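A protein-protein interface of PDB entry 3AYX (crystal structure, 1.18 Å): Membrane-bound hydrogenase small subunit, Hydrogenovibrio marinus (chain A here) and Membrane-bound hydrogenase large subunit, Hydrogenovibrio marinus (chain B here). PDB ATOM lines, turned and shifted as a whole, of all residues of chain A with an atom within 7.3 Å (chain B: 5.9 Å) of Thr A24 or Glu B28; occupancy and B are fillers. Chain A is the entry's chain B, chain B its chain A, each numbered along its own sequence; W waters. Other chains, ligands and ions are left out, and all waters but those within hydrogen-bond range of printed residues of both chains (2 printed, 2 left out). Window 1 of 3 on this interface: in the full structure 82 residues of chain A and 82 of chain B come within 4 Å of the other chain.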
ATOM      1  N   HIS A  19      -0.107  -9.708   9.201  1.00  0.00           N
ATOM      2  CA  HIS A  19       1.294  -9.417   9.432  1.00  0.00           C
ATOM      3  C   HIS A  19       1.633  -9.648  10.891  1.00  0.00           C
ATOM      4  O   HIS A  19       1.108  -8.999  11.791  1.00  0.00           O
ATOM      5  CB  HIS A  19       1.642  -7.952   9.107  1.00  0.00           C
ATOM      6  CG  HIS A  19       1.528  -7.567   7.668  1.00  0.00           C
ATOM      7  ND1 HIS A  19       2.615  -7.402   6.896  1.00  0.00           N
ATOM      8  CD2 HIS A  19       0.461  -7.268   6.899  1.00  0.00           C
ATOM      9  CE1 HIS A  19       2.215  -7.016   5.658  1.00  0.00           C
ATOM     10  NE2 HIS A  19       0.910  -6.942   5.656  1.00  0.00           N
ATOM     11  N   GLY A  20       2.536 -10.589  11.146  1.00  0.00           N
ATOM     12  CA  GLY A  20       3.024 -10.887  12.484  1.00  0.00           C
ATOM     13  C   GLY A  20       4.380 -10.222  12.728  1.00  0.00           C
ATOM     14  O   GLY A  20       4.626  -9.094  12.262  1.00  0.00           O
ATOM     15  N   LEU A  21       5.266 -10.914  13.418  1.00  0.00           N
ATOM     16  CA  LEU A  21       6.666 -10.489  13.475  1.00  0.00           C
ATOM     17  C   LEU A  21       7.280 -10.718  12.112  1.00  0.00           C
ATOM     18  O   LEU A  21       7.175 -11.819  11.561  1.00  0.00           O
ATOM     19  CB  LEU A  21       7.410 -11.283  14.503  1.00  0.00           C
ATOM     20  CG  LEU A  21       7.136 -10.993  15.967  1.00  0.00           C
ATOM     21  CD1 LEU A  21       8.028 -11.883  16.834  1.00  0.00           C
ATOM     22  CD2 LEU A  21       7.314  -9.513  16.290  1.00  0.00           C
ATOM     23  N   GLU A  22       7.900  -9.677  11.540  1.00  0.00           N
ATOM     24  CA  GLU A  22       8.217  -9.639  10.138  1.00  0.00           C
ATOM     25  C   GLU A  22       9.223  -8.524   9.891  1.00  0.00           C
ATOM     26  O   GLU A  22       9.432  -7.678  10.748  1.00  0.00           O
ATOM     27  CB  GLU A  22       6.977  -9.263   9.329  1.00  0.00           C
ATOM     28  CG  GLU A  22       6.500  -7.838   9.633  1.00  0.00           C
ATOM     29  CD  GLU A  22       5.292  -7.307   8.977  1.00  0.00           C
ATOM     30  OE1 GLU A  22       4.998  -7.785   7.886  1.00  0.00           O
ATOM     31  OE2 GLU A  22       4.674  -6.370   9.569  1.00  0.00           O
ATOM     32  N   CYS A  23       9.759  -8.474   8.673  1.00  0.00           N
ATOM     33  CA  CYS A  23      10.490  -7.305   8.196  1.00  0.00           C
ATOM     34  C   CYS A  23       9.757  -6.611   7.038  1.00  0.00           C
ATOM     35  O   CYS A  23      10.191  -5.542   6.600  1.00  0.00           O
ATOM     36  CB  CYS A  23      11.956  -7.620   7.775  1.00  0.00           C
ATOM     37  SG  CYS A  23      12.084  -8.321   6.077  1.00  0.00           S
ATOM     38  N   THR A  24       8.667  -7.221   6.531  1.00  0.00           N
ATOM     39  CA  THR A  24       7.863  -6.723   5.402  1.00  0.00           C
ATOM     40  C   THR A  24       8.464  -7.032   4.059  1.00  0.00           C
ATOM     41  O   THR A  24       7.992  -6.596   3.006  1.00  0.00           O
ATOM     42  CB  THR A  24       7.406  -5.261   5.574  1.00  0.00           C
ATOM     43  OG1 THR A  24       7.035  -5.109   6.958  1.00  0.00           O
ATOM     44  CG2 THR A  24       6.251  -4.842   4.711  1.00  0.00           C
ATOM     45  N   CYS A  25       9.486  -7.884   4.004  1.00  0.00           N
ATOM     46  CA  CYS A  25      10.096  -8.214   2.713  1.00  0.00           C
ATOM     47  C   CYS A  25       9.145  -8.988   1.822  1.00  0.00           C
ATOM     48  O   CYS A  25       9.313  -8.928   0.601  1.00  0.00           O
ATOM     49  CB  CYS A  25      11.414  -8.997   2.824  1.00  0.00           C
ATOM     50  SG  CYS A  25      11.492 -10.651   3.651  1.00  0.00           S
ATOM     51  N   CYS A  26       8.175  -9.724   2.374  1.00  0.00           N
ATOM     52  CA  CYS A  26       7.282 -10.524   1.566  1.00  0.00           C
ATOM     53  C   CYS A  26       6.256  -9.660   0.860  1.00  0.00           C
ATOM     54  O   CYS A  26       6.033  -9.849  -0.363  1.00  0.00           O
ATOM     55  CB  CYS A  26       6.661 -11.630   2.403  1.00  0.00           C
ATOM     56  SG  CYS A  26       7.934 -12.827   2.988  1.00  0.00           S
ATOM     57  N   SER A  27       5.687  -8.645   1.535  1.00  0.00           N
ATOM     58  CA  SER A  27       4.830  -7.656   0.875  1.00  0.00           C
ATOM     59  C   SER A  27       5.586  -6.921  -0.205  1.00  0.00           C
ATOM     60  O   SER A  27       5.059  -6.640  -1.309  1.00  0.00           O
ATOM     61  CB  SER A  27       4.274  -6.664   1.849  1.00  0.00           C
ATOM     62  OG  SER A  27       3.206  -7.189   2.592  1.00  0.00           O
ATOM     63  N   GLU A  28       6.817  -6.517   0.126  1.00  0.00           N
ATOM     64  CA  GLU A  28       7.637  -5.821  -0.842  1.00  0.00           C
ATOM     65  C   GLU A  28       7.886  -6.632  -2.094  1.00  0.00           C
ATOM     66  O   GLU A  28       7.775  -6.177  -3.221  1.00  0.00           O
ATOM     67  CB  GLU A  28       8.936  -5.357  -0.184  1.00  0.00           C
ATOM     68  CG  GLU A  28       8.695  -4.153   0.766  1.00  0.00           C
ATOM     69  CD  GLU A  28       8.532  -2.830   0.060  1.00  0.00           C
ATOM     70  OE1 GLU A  28       8.661  -2.689  -1.158  1.00  0.00           O
ATOM     71  OE2 GLU A  28       8.377  -1.848   0.860  1.00  0.00           O
ATOM     72  N   SER A  29       8.255  -7.900  -1.876  1.00  0.00           N
ATOM     73  CA  SER A  29       8.474  -8.750  -3.063  1.00  0.00           C
ATOM     74  C   SER A  29       7.211  -8.839  -3.895  1.00  0.00           C
ATOM     75  O   SER A  29       7.288  -8.762  -5.131  1.00  0.00           O
ATOM     76  CB  SER A  29       8.967 -10.128  -2.632  1.00  0.00           C
ATOM     77  OG  SER A  29       9.409 -10.775  -3.812  1.00  0.00           O
ATOM     78  N   PHE A  30       6.068  -9.063  -3.261  1.00  0.00           N
ATOM     79  CA  PHE A  30       4.815  -9.225  -3.999  1.00  0.00           C
ATOM     80  C   PHE A  30       4.587  -8.109  -4.973  1.00  0.00           C
ATOM     81  O   PHE A  30       4.222  -8.344  -6.134  1.00  0.00           O
ATOM     82  CB  PHE A  30       3.687  -9.318  -2.964  1.00  0.00           C
ATOM     83  CG  PHE A  30       2.335  -9.615  -3.571  1.00  0.00           C
ATOM     84  CD1 PHE A  30       1.941 -10.945  -3.779  1.00  0.00           C
ATOM     85  CD2 PHE A  30       1.486  -8.602  -3.881  1.00  0.00           C
ATOM     86  CE1 PHE A  30       0.701 -11.273  -4.277  1.00  0.00           C
ATOM     87  CE2 PHE A  30       0.194  -8.952  -4.367  1.00  0.00           C
ATOM     88  CZ  PHE A  30      -0.194 -10.237  -4.573  1.00  0.00           C
ATOM     89  N   ARG A  32       6.683  -6.325  -6.523  1.00  0.00           N
ATOM     90  CA  ARG A  32       7.604  -6.324  -7.622  1.00  0.00           C
ATOM     91  C   ARG A  32       7.159  -7.136  -8.828  1.00  0.00           C
ATOM     92  O   ARG A  32       7.806  -7.126  -9.868  1.00  0.00           O
ATOM     93  CB  ARG A  32       8.978  -6.860  -7.220  1.00  0.00           C
ATOM     94  CG  ARG A  32       9.611  -6.201  -6.020  1.00  0.00           C
ATOM     95  CD  ARG A  32       9.960  -4.706  -6.271  1.00  0.00           C
ATOM     96  NE  ARG A  32      10.724  -4.279  -5.116  1.00  0.00           N
ATOM     97  CZ  ARG A  32      10.243  -3.836  -3.951  1.00  0.00           C
ATOM     98  NH1 ARG A  32       9.003  -3.399  -3.851  1.00  0.00           N
ATOM     99  NH2 ARG A  32      10.977  -3.747  -2.867  1.00  0.00           N
ATOM    100  N   ASP A  51      -4.768  -5.565   4.876  1.00  0.00           N
ATOM    101  CA  ASP A  51      -3.330  -5.639   4.617  1.00  0.00           C
ATOM    102  C   ASP A  51      -2.674  -4.436   5.253  1.00  0.00           C
ATOM    103  O   ASP A  51      -2.860  -3.303   4.678  1.00  0.00           O
ATOM    104  CB  ASP A  51      -3.011  -5.697   3.146  1.00  0.00           C
ATOM    105  CG  ASP A  51      -1.534  -5.932   2.801  1.00  0.00           C
ATOM    106  OD1 ASP A  51      -0.683  -5.886   3.652  1.00  0.00           O
ATOM    107  OD2 ASP A  51      -1.264  -6.169   1.557  1.00  0.00           O
ATOM    108  N   ASP A  52      -1.940  -4.553   6.357  1.00  0.00           N
ATOM    109  CA  ASP A  52      -1.442  -3.434   7.105  1.00  0.00           C
ATOM    110  C   ASP A  52      -0.642  -2.503   6.230  1.00  0.00           C
ATOM    111  O   ASP A  52      -0.665  -1.278   6.425  1.00  0.00           O
ATOM    112  CB  ASP A  52      -0.531  -3.960   8.229  1.00  0.00           C
ATOM    113  CG  ASP A  52      -1.079  -5.121   9.011  1.00  0.00           C
ATOM    114  OD1 ASP A  52      -0.924  -5.101  10.238  1.00  0.00           O
ATOM    115  OD2 ASP A  52      -1.675  -6.153   8.487  1.00  0.00           O
ATOM    116  N   THR A  53       0.114  -3.071   5.279  1.00  0.00           N
ATOM    117  CA  THR A  53       1.052  -2.197   4.577  1.00  0.00           C
ATOM    118  C   THR A  53       0.365  -1.148   3.692  1.00  0.00           C
ATOM    119  O   THR A  53       0.894  -0.041   3.576  1.00  0.00           O
ATOM    120  CB  THR A  53       2.026  -3.031   3.727  1.00  0.00           C
ATOM    121  OG1 THR A  53       2.560  -4.118   4.506  1.00  0.00           O
ATOM    122  CG2 THR A  53       3.218  -2.206   3.218  1.00  0.00           C
ATOM    123  N   GLU A  82       1.998 -13.086   6.484  1.00  0.00           N
ATOM    124  CA  GLU A  82       3.377 -12.626   6.459  1.00  0.00           C
ATOM    125  C   GLU A  82       3.833 -12.540   7.896  1.00  0.00           C
ATOM    126  O   GLU A  82       3.100 -12.062   8.782  1.00  0.00           O
ATOM    127  CB  GLU A  82       3.465 -11.323   5.708  1.00  0.00           C
ATOM    128  CG  GLU A  82       4.799 -10.647   5.620  1.00  0.00           C
ATOM    129  CD  GLU A  82       4.848  -9.523   4.629  1.00  0.00           C
ATOM    130  OE1 GLU A  82       3.745  -9.140   4.136  1.00  0.00           O
ATOM    131  OE2 GLU A  82       5.918  -9.007   4.319  1.00  0.00           O
ATOM    132  N   GLY A  83       5.076 -12.905   8.149  1.00  0.00           N
ATOM    133  CA  GLY A  83       5.558 -12.885   9.513  1.00  0.00           C
ATOM    134  C   GLY A  83       5.012 -14.075  10.326  1.00  0.00           C
ATOM    135  O   GLY A  83       4.436 -15.009   9.751  1.00  0.00           O
ATOM    136  N   CYS A 121       9.351 -16.492   7.130  1.00  0.00           N
ATOM    137  CA  CYS A 121       8.817 -16.237   8.484  1.00  0.00           C
ATOM    138  C   CYS A 121       7.589 -17.107   8.734  1.00  0.00           C
ATOM    139  O   CYS A 121       7.491 -17.809   9.731  1.00  0.00           O
ATOM    140  CB  CYS A 121       8.350 -14.762   8.657  1.00  0.00           C
ATOM    141  SG  CYS A 121       9.660 -13.580   8.951  1.00  0.00           S
ATOM    142  N   PRO A 159      12.828 -12.777   0.818  1.00  0.00           N
ATOM    143  CA  PRO A 159      11.443 -13.200   0.595  1.00  0.00           C
ATOM    144  C   PRO A 159      11.366 -14.201  -0.552  1.00  0.00           C
ATOM    145  O   PRO A 159      12.380 -14.475  -1.196  1.00  0.00           O
ATOM    146  CB  PRO A 159      10.742 -11.901   0.237  1.00  0.00           C
ATOM    147  CG  PRO A 159      11.776 -11.158  -0.564  1.00  0.00           C
ATOM    148  CD  PRO A 159      13.124 -11.584   0.021  1.00  0.00           C
ATOM    149  N   ARG B  26      -0.354   1.460   7.184  1.00  0.00           N
ATOM    150  CA  ARG B  26       0.434   2.187   6.185  1.00  0.00           C
ATOM    151  C   ARG B  26       1.768   2.718   6.795  1.00  0.00           C
ATOM    152  O   ARG B  26       2.176   3.846   6.590  1.00  0.00           O
ATOM    153  CB  ARG B  26      -0.351   3.263   5.474  1.00  0.00           C
ATOM    154  CG  ARG B  26      -1.236   2.678   4.380  1.00  0.00           C
ATOM    155  CD  ARG B  26      -2.087   3.633   3.617  1.00  0.00           C
ATOM    156  NE  ARG B  26      -3.099   4.201   4.477  1.00  0.00           N
ATOM    157  CZ  ARG B  26      -3.194   5.472   4.870  1.00  0.00           C
ATOM    158  NH1 ARG B  26      -2.283   6.437   4.549  1.00  0.00           N
ATOM    159  NH2 ARG B  26      -4.224   5.818   5.615  1.00  0.00           N
ATOM    160  N   ILE B  27       2.394   1.801   7.536  1.00  0.00           N
ATOM    161  CA  ILE B  27       3.721   1.850   8.008  1.00  0.00           C
ATOM    162  C   ILE B  27       4.349   0.498   7.745  1.00  0.00           C
ATOM    163  O   ILE B  27       3.647  -0.442   7.377  1.00  0.00           O
ATOM    164  CB  ILE B  27       3.849   2.153   9.510  1.00  0.00           C
ATOM    165  CG1 ILE B  27       3.096   1.079  10.299  1.00  0.00           C
ATOM    166  CG2 ILE B  27       3.322   3.565   9.780  1.00  0.00           C
ATOM    167  CD1 ILE B  27       3.321   1.090  11.737  1.00  0.00           C
ATOM    168  N   GLU B  28       5.684   0.399   7.928  1.00  0.00           N
ATOM    169  CA  GLU B  28       6.270  -0.914   8.035  1.00  0.00           C
ATOM    170  C   GLU B  28       6.082  -1.324   9.493  1.00  0.00           C
ATOM    171  O   GLU B  28       6.443  -0.608  10.392  1.00  0.00           O
ATOM    172  CB  GLU B  28       7.745  -0.887   7.667  1.00  0.00           C
ATOM    173  CG  GLU B  28       8.493  -2.266   7.628  1.00  0.00           C
ATOM    174  CD  GLU B  28       8.587  -3.113   8.799  1.00  0.00           C
ATOM    175  OE1 GLU B  28       8.727  -2.337   9.862  1.00  0.00           O
ATOM    176  OE2 GLU B  28       8.279  -4.308   9.080  1.00  0.00           O
ATOM    177  N   GLY B  29       5.643  -2.557   9.653  1.00  0.00           N
ATOM    178  CA  GLY B  29       5.623  -3.152  10.993  1.00  0.00           C
ATOM    179  C   GLY B  29       4.429  -2.773  11.794  1.00  0.00           C
ATOM    180  O   GLY B  29       3.386  -2.575  11.223  1.00  0.00           O
ATOM    181  N   HIS B  30       4.584  -2.647  13.105  1.00  0.00           N
ATOM    182  CA  HIS B  30       3.450  -2.491  14.007  1.00  0.00           C
ATOM    183  C   HIS B  30       3.701  -1.358  14.991  1.00  0.00           C
ATOM    184  O   HIS B  30       4.761  -1.260  15.601  1.00  0.00           O
ATOM    185  CB  HIS B  30       3.209  -3.771  14.788  1.00  0.00           C
ATOM    186  CG  HIS B  30       3.073  -4.952  13.899  1.00  0.00           C
ATOM    187  ND1 HIS B  30       1.965  -5.105  13.083  1.00  0.00           N
ATOM    188  CD2 HIS B  30       3.818  -6.014  13.653  1.00  0.00           C
ATOM    189  CE1 HIS B  30       2.059  -6.204  12.377  1.00  0.00           C
ATOM    190  NE2 HIS B  30       3.159  -6.799  12.718  1.00  0.00           N
ATOM    191  N   MET B  52       6.144  -4.252  18.344  1.00  0.00           N
ATOM    192  CA  MET B  52       6.803  -5.499  18.003  1.00  0.00           C
ATOM    193  C   MET B  52       8.248  -5.490  18.477  1.00  0.00           C
ATOM    194  O   MET B  52       8.876  -4.442  18.555  1.00  0.00           O
ATOM    195  CB  MET B  52       6.768  -5.786  16.495  1.00  0.00           C
ATOM    196  CG  MET B  52       7.477  -4.706  15.673  1.00  0.00           C
ATOM    197  SD  MET B  52       7.393  -4.881  13.902  1.00  0.00           S
ATOM    198  CE  MET B  52       8.376  -6.370  13.720  1.00  0.00           C
ATOM    199  N   ILE B  75      16.395  -7.005   9.454  1.00  0.00           N
ATOM    200  CA  ILE B  75      15.654  -6.068  10.278  1.00  0.00           C
ATOM    201  C   ILE B  75      14.514  -5.432   9.512  1.00  0.00           C
ATOM    202  O   ILE B  75      13.458  -5.161  10.059  1.00  0.00           O
ATOM    203  CB  ILE B  75      16.612  -5.026  10.915  1.00  0.00           C
ATOM    204  CG1 ILE B  75      17.515  -5.678  11.936  1.00  0.00           C
ATOM    205  CG2 ILE B  75      15.874  -3.833  11.470  1.00  0.00           C
ATOM    206  CD1 ILE B  75      18.679  -4.804  12.421  1.00  0.00           C
ATOM    207  N   CYS B  76      14.733  -5.215   8.203  1.00  0.00           N
ATOM    208  CA  CYS B  76      13.748  -4.470   7.449  1.00  0.00           C
ATOM    209  C   CYS B  76      13.827  -4.765   5.969  1.00  0.00           C
ATOM    210  O   CYS B  76      14.848  -4.666   5.319  1.00  0.00           O
ATOM    211  CB  CYS B  76      13.965  -3.019   7.636  1.00  0.00           C
ATOM    212  SG  CYS B  76      12.514  -2.105   6.975  1.00  0.00           S
ATOM    213  N   GLY B  77      12.615  -5.082   5.427  1.00  0.00           N
ATOM    214  CA  GLY B  77      12.428  -5.363   4.006  1.00  0.00           C
ATOM    215  C   GLY B  77      12.076  -4.173   3.187  1.00  0.00           C
ATOM    216  O   GLY B  77      12.086  -4.285   1.967  1.00  0.00           O
ATOM    217  N   VAL B  78      11.767  -3.071   3.829  1.00  0.00           N
ATOM    218  CA  VAL B  78      11.407  -1.783   3.224  1.00  0.00           C
ATOM    219  C   VAL B  78      12.716  -1.048   2.986  1.00  0.00           C
ATOM    220  O   VAL B  78      13.093  -0.785   1.830  1.00  0.00           O
ATOM    221  CB  VAL B  78      10.366  -1.063   4.053  1.00  0.00           C
ATOM    222  CG1 VAL B  78      10.028   0.221   3.392  1.00  0.00           C
ATOM    223  CG2 VAL B  78       9.093  -1.871   4.260  1.00  0.00           C
ATOM    224  N   LEU B 126       2.011   4.467   0.911  1.00  0.00           N
ATOM    225  CA  LEU B 126       1.836   4.597   2.346  1.00  0.00           C
ATOM    226  C   LEU B 126       1.208   5.916   2.757  1.00  0.00           C
ATOM    227  O   LEU B 126       0.326   5.974   3.593  1.00  0.00           O
ATOM    228  CB  LEU B 126       3.158   4.379   3.064  1.00  0.00           C
ATOM    229  CG  LEU B 126       3.935   3.091   2.861  1.00  0.00           C
ATOM    230  CD1 LEU B 126       4.838   2.799   4.066  1.00  0.00           C
ATOM    231  CD2 LEU B 126       3.054   1.884   2.602  1.00  0.00           C
ATOM    232  N   PRO B 229      13.572  -7.706  -2.732  1.00  0.00           N
ATOM    233  CA  PRO B 229      14.305  -7.307  -1.530  1.00  0.00           C
ATOM    234  C   PRO B 229      15.469  -8.217  -1.190  1.00  0.00           C
ATOM    235  O   PRO B 229      15.647  -9.325  -1.668  1.00  0.00           O
ATOM    236  CB  PRO B 229      13.232  -7.435  -0.410  1.00  0.00           C
ATOM    237  CG  PRO B 229      11.930  -7.243  -1.132  1.00  0.00           C
ATOM    238  CD  PRO B 229      12.133  -7.868  -2.470  1.00  0.00           C
ATOM    239  N   ARG B 523      15.151   6.771   6.256  1.00  0.00           N
ATOM    240  CA  ARG B 523      14.403   7.404   7.347  1.00  0.00           C
ATOM    241  C   ARG B 523      15.258   8.257   8.254  1.00  0.00           C
ATOM    242  O   ARG B 523      14.746   8.823   9.189  1.00  0.00           O
ATOM    243  CB  ARG B 523      13.586   6.381   8.113  1.00  0.00           C
ATOM    244  CG  ARG B 523      12.467   5.815   7.223  1.00  0.00           C
ATOM    245  CD  ARG B 523      12.010   4.440   7.675  1.00  0.00           C
ATOM    246  NE  ARG B 523      10.996   3.981   6.698  1.00  0.00           N
ATOM    247  CZ  ARG B 523      11.257   3.456   5.500  1.00  0.00           C
ATOM    248  NH1 ARG B 523      12.485   3.175   5.171  1.00  0.00           N
ATOM    249  NH2 ARG B 523      10.276   3.173   4.709  1.00  0.00           N
ATOM    250  N   PRO B 589       7.427   5.989   9.329  1.00  0.00           N
ATOM    251  CA  PRO B 589       7.825   5.085  10.417  1.00  0.00           C
ATOM    252  C   PRO B 589       8.135   3.660   9.940  1.00  0.00           C
ATOM    253  O   PRO B 589       7.332   3.048   9.205  1.00  0.00           O
ATOM    254  CB  PRO B 589       6.578   5.110  11.308  1.00  0.00           C
ATOM    255  CG  PRO B 589       5.894   6.354  10.996  1.00  0.00           C
ATOM    256  CD  PRO B 589       6.080   6.521   9.508  1.00  0.00           C
ATOM    257  N   CYS B 590       9.253   3.136  10.382  1.00  0.00           N
ATOM    258  CA  CYS B 590       9.681   1.761  10.106  1.00  0.00           C
ATOM    259  C   CYS B 590       9.817   1.073  11.437  1.00  0.00           C
ATOM    260  O   CYS B 590      10.801   1.224  12.170  1.00  0.00           O
ATOM    261  CB  CYS B 590      10.983   1.791   9.323  1.00  0.00           C
ATOM    262  SG  CYS B 590      11.215   0.133   8.560  1.00  0.00           S
ATOM    263  N   LEU B 591       8.725   0.384  11.835  1.00  0.00           N
ATOM    264  CA  LEU B 591       8.675  -0.101  13.211  1.00  0.00           C
ATOM    265  C   LEU B 591       9.480  -1.355  13.435  1.00  0.00           C
ATOM    266  O   LEU B 591       9.949  -1.589  14.543  1.00  0.00           O
ATOM    267  CB  LEU B 591       7.210  -0.273  13.599  1.00  0.00           C
ATOM    268  CG  LEU B 591       6.527   1.001  14.090  1.00  0.00           C
ATOM    269  CD1 LEU B 591       6.999   1.394  15.457  1.00  0.00           C
ATOM    270  CD2 LEU B 591       6.617   2.176  13.104  1.00  0.00           C
ATOM    271  N   ALA B 592       9.638  -2.171  12.428  1.00  0.00           N
ATOM    272  CA  ALA B 592      10.517  -3.345  12.521  1.00  0.00           C
ATOM    273  C   ALA B 592      11.929  -2.852  12.683  1.00  0.00           C
ATOM    274  O   ALA B 592      12.708  -3.334  13.534  1.00  0.00           O
ATOM    275  CB  ALA B 592      10.369  -4.263  11.306  1.00  0.00           C
ATOM    276  N   CYS B 593      12.336  -1.833  11.914  1.00  0.00           N
ATOM    277  CA  CYS B 593      13.594  -1.191  12.132  1.00  0.00           C
ATOM    278  C   CYS B 593      13.730  -0.647  13.556  1.00  0.00           C
ATOM    279  O   CYS B 593      14.764  -0.821  14.149  1.00  0.00           O
ATOM    280  CB  CYS B 593      13.867   0.104  11.255  1.00  0.00           C
ATOM    281  SG  CYS B 593      14.522  -0.376   9.662  1.00  0.00           S
HETATM  282  O   HOH W   1       3.768  -3.384   6.918  1.00  0.00           O
HETATM  283  O   HOH W   2       2.945  -4.648   9.071  1.00  0.00           O
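Of the 20 printed residues of chain A, 12 touch a printed residue of chain B. Hydrophobic or aromatic side chains of chain A within 4 Å of the printed part of chain B: His A19, Leu A21 and Pro A159. Of the 18 printed residues of chain B, 12 touch a printed residue of chain A. Hydrophobic or aromatic side chains of chain B that line the printed part of chain A: His B30, Met B52, Val B78, Leu B126, Pro B229 and Ala B592.
Printed residues of chain B within 4 Å of Thr A24: Glu B28 and Gly B29. Printed residues of chain A within 4 Å of Glu B28: Glu A22, Cys A23 and Thr A24. Of the printed residues of chain A, Met B52 touches Leu A21 and Glu A22. Of the printed residues of chain A, Leu B126 touches Thr A53 (3.1 Å). Of the printed residues of chain B, Glu A22 touches Glu B28, Gly B29, His B30, Met B52 and Ala B592. Printed residues of chain A within 4 Å of Ala B592: Glu A22 (3.6 Å). Gly A83 touches none of the printed residues of chain B. Leu B591 touches none of the printed residues of chain A. The nearest printed residue of chain A that does not touch His B30 is Leu A21 (4.7 Å).
NE2 of His B30 lies within hydrogen-bond range of O of Gly A20, at 2.8 Å. The backbone NH of Arg B26 sits at hydrogen-bond distance from the backbone carbonyl oxygen of Asp A52, at 2.9 Å. O of Cys A23 sits at hydrogen-bond distance from N of Gly B77 (2.7 Å). The backbone carbonyl oxygen (O) of His A19 sits close to a ring nitrogen (NE2) of His B30. OE2 of Glu B28 is in hydrogen-bond range of OG1 of Thr A24, at 2.6 Å. O of Cys A23 sits close to OE2 of Glu B28, at 3.4 Å.
Water W2 bridges OE2 of Glu A22 (2.5 Å) and O of Gly B29 (3.0 Å). Water W1 lies within hydrogen-bond range of OG1 of Thr A53, O of Ile B27 and N of Gly B29.
Leu A21 touches Met B52. Glu A22 touches Glu B28. Glu A22 touches Gly B29. O of Glu A22 touches CB of Ala B592 (3.6 Å). Cys A23 touches Cys B76 (CB to CA, 3.6 Å). N of Gly B29 touches OG1 of Thr A24, 3.96 Å away. Cys A25 touches Gly B77 (N to CA, 3.9 Å). O of Gly B77 touches CG of Glu A28, 3.6 Å away. OE2 of Glu A28 touches CG2 of Val B78, at 3.5 Å. O of Pro B229 touches CD of Pro A159, 3.8 Å away.
NE2 of His A19 is in hydrogen-bond range of OD1 of Asp A51 (2.8 Å). SD of Met B52 sits at hydrogen-bond distance from N of His B30, 3.7 Å away. The backbone NH of Gly A20 lies within hydrogen-bond range of the backbone carbonyl oxygen of Glu A82 (2.8 Å). N of Glu B28 lies within hydrogen-bond range of O of Pro B589 (3.4 Å). A ring nitrogen (NE2) of His A19 sits close to the side-chain hydroxyl of Thr A53 (3.5 Å). OE1 of Glu B28 is in hydrogen-bond range of N of Ala B592, at 2.7 Å.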
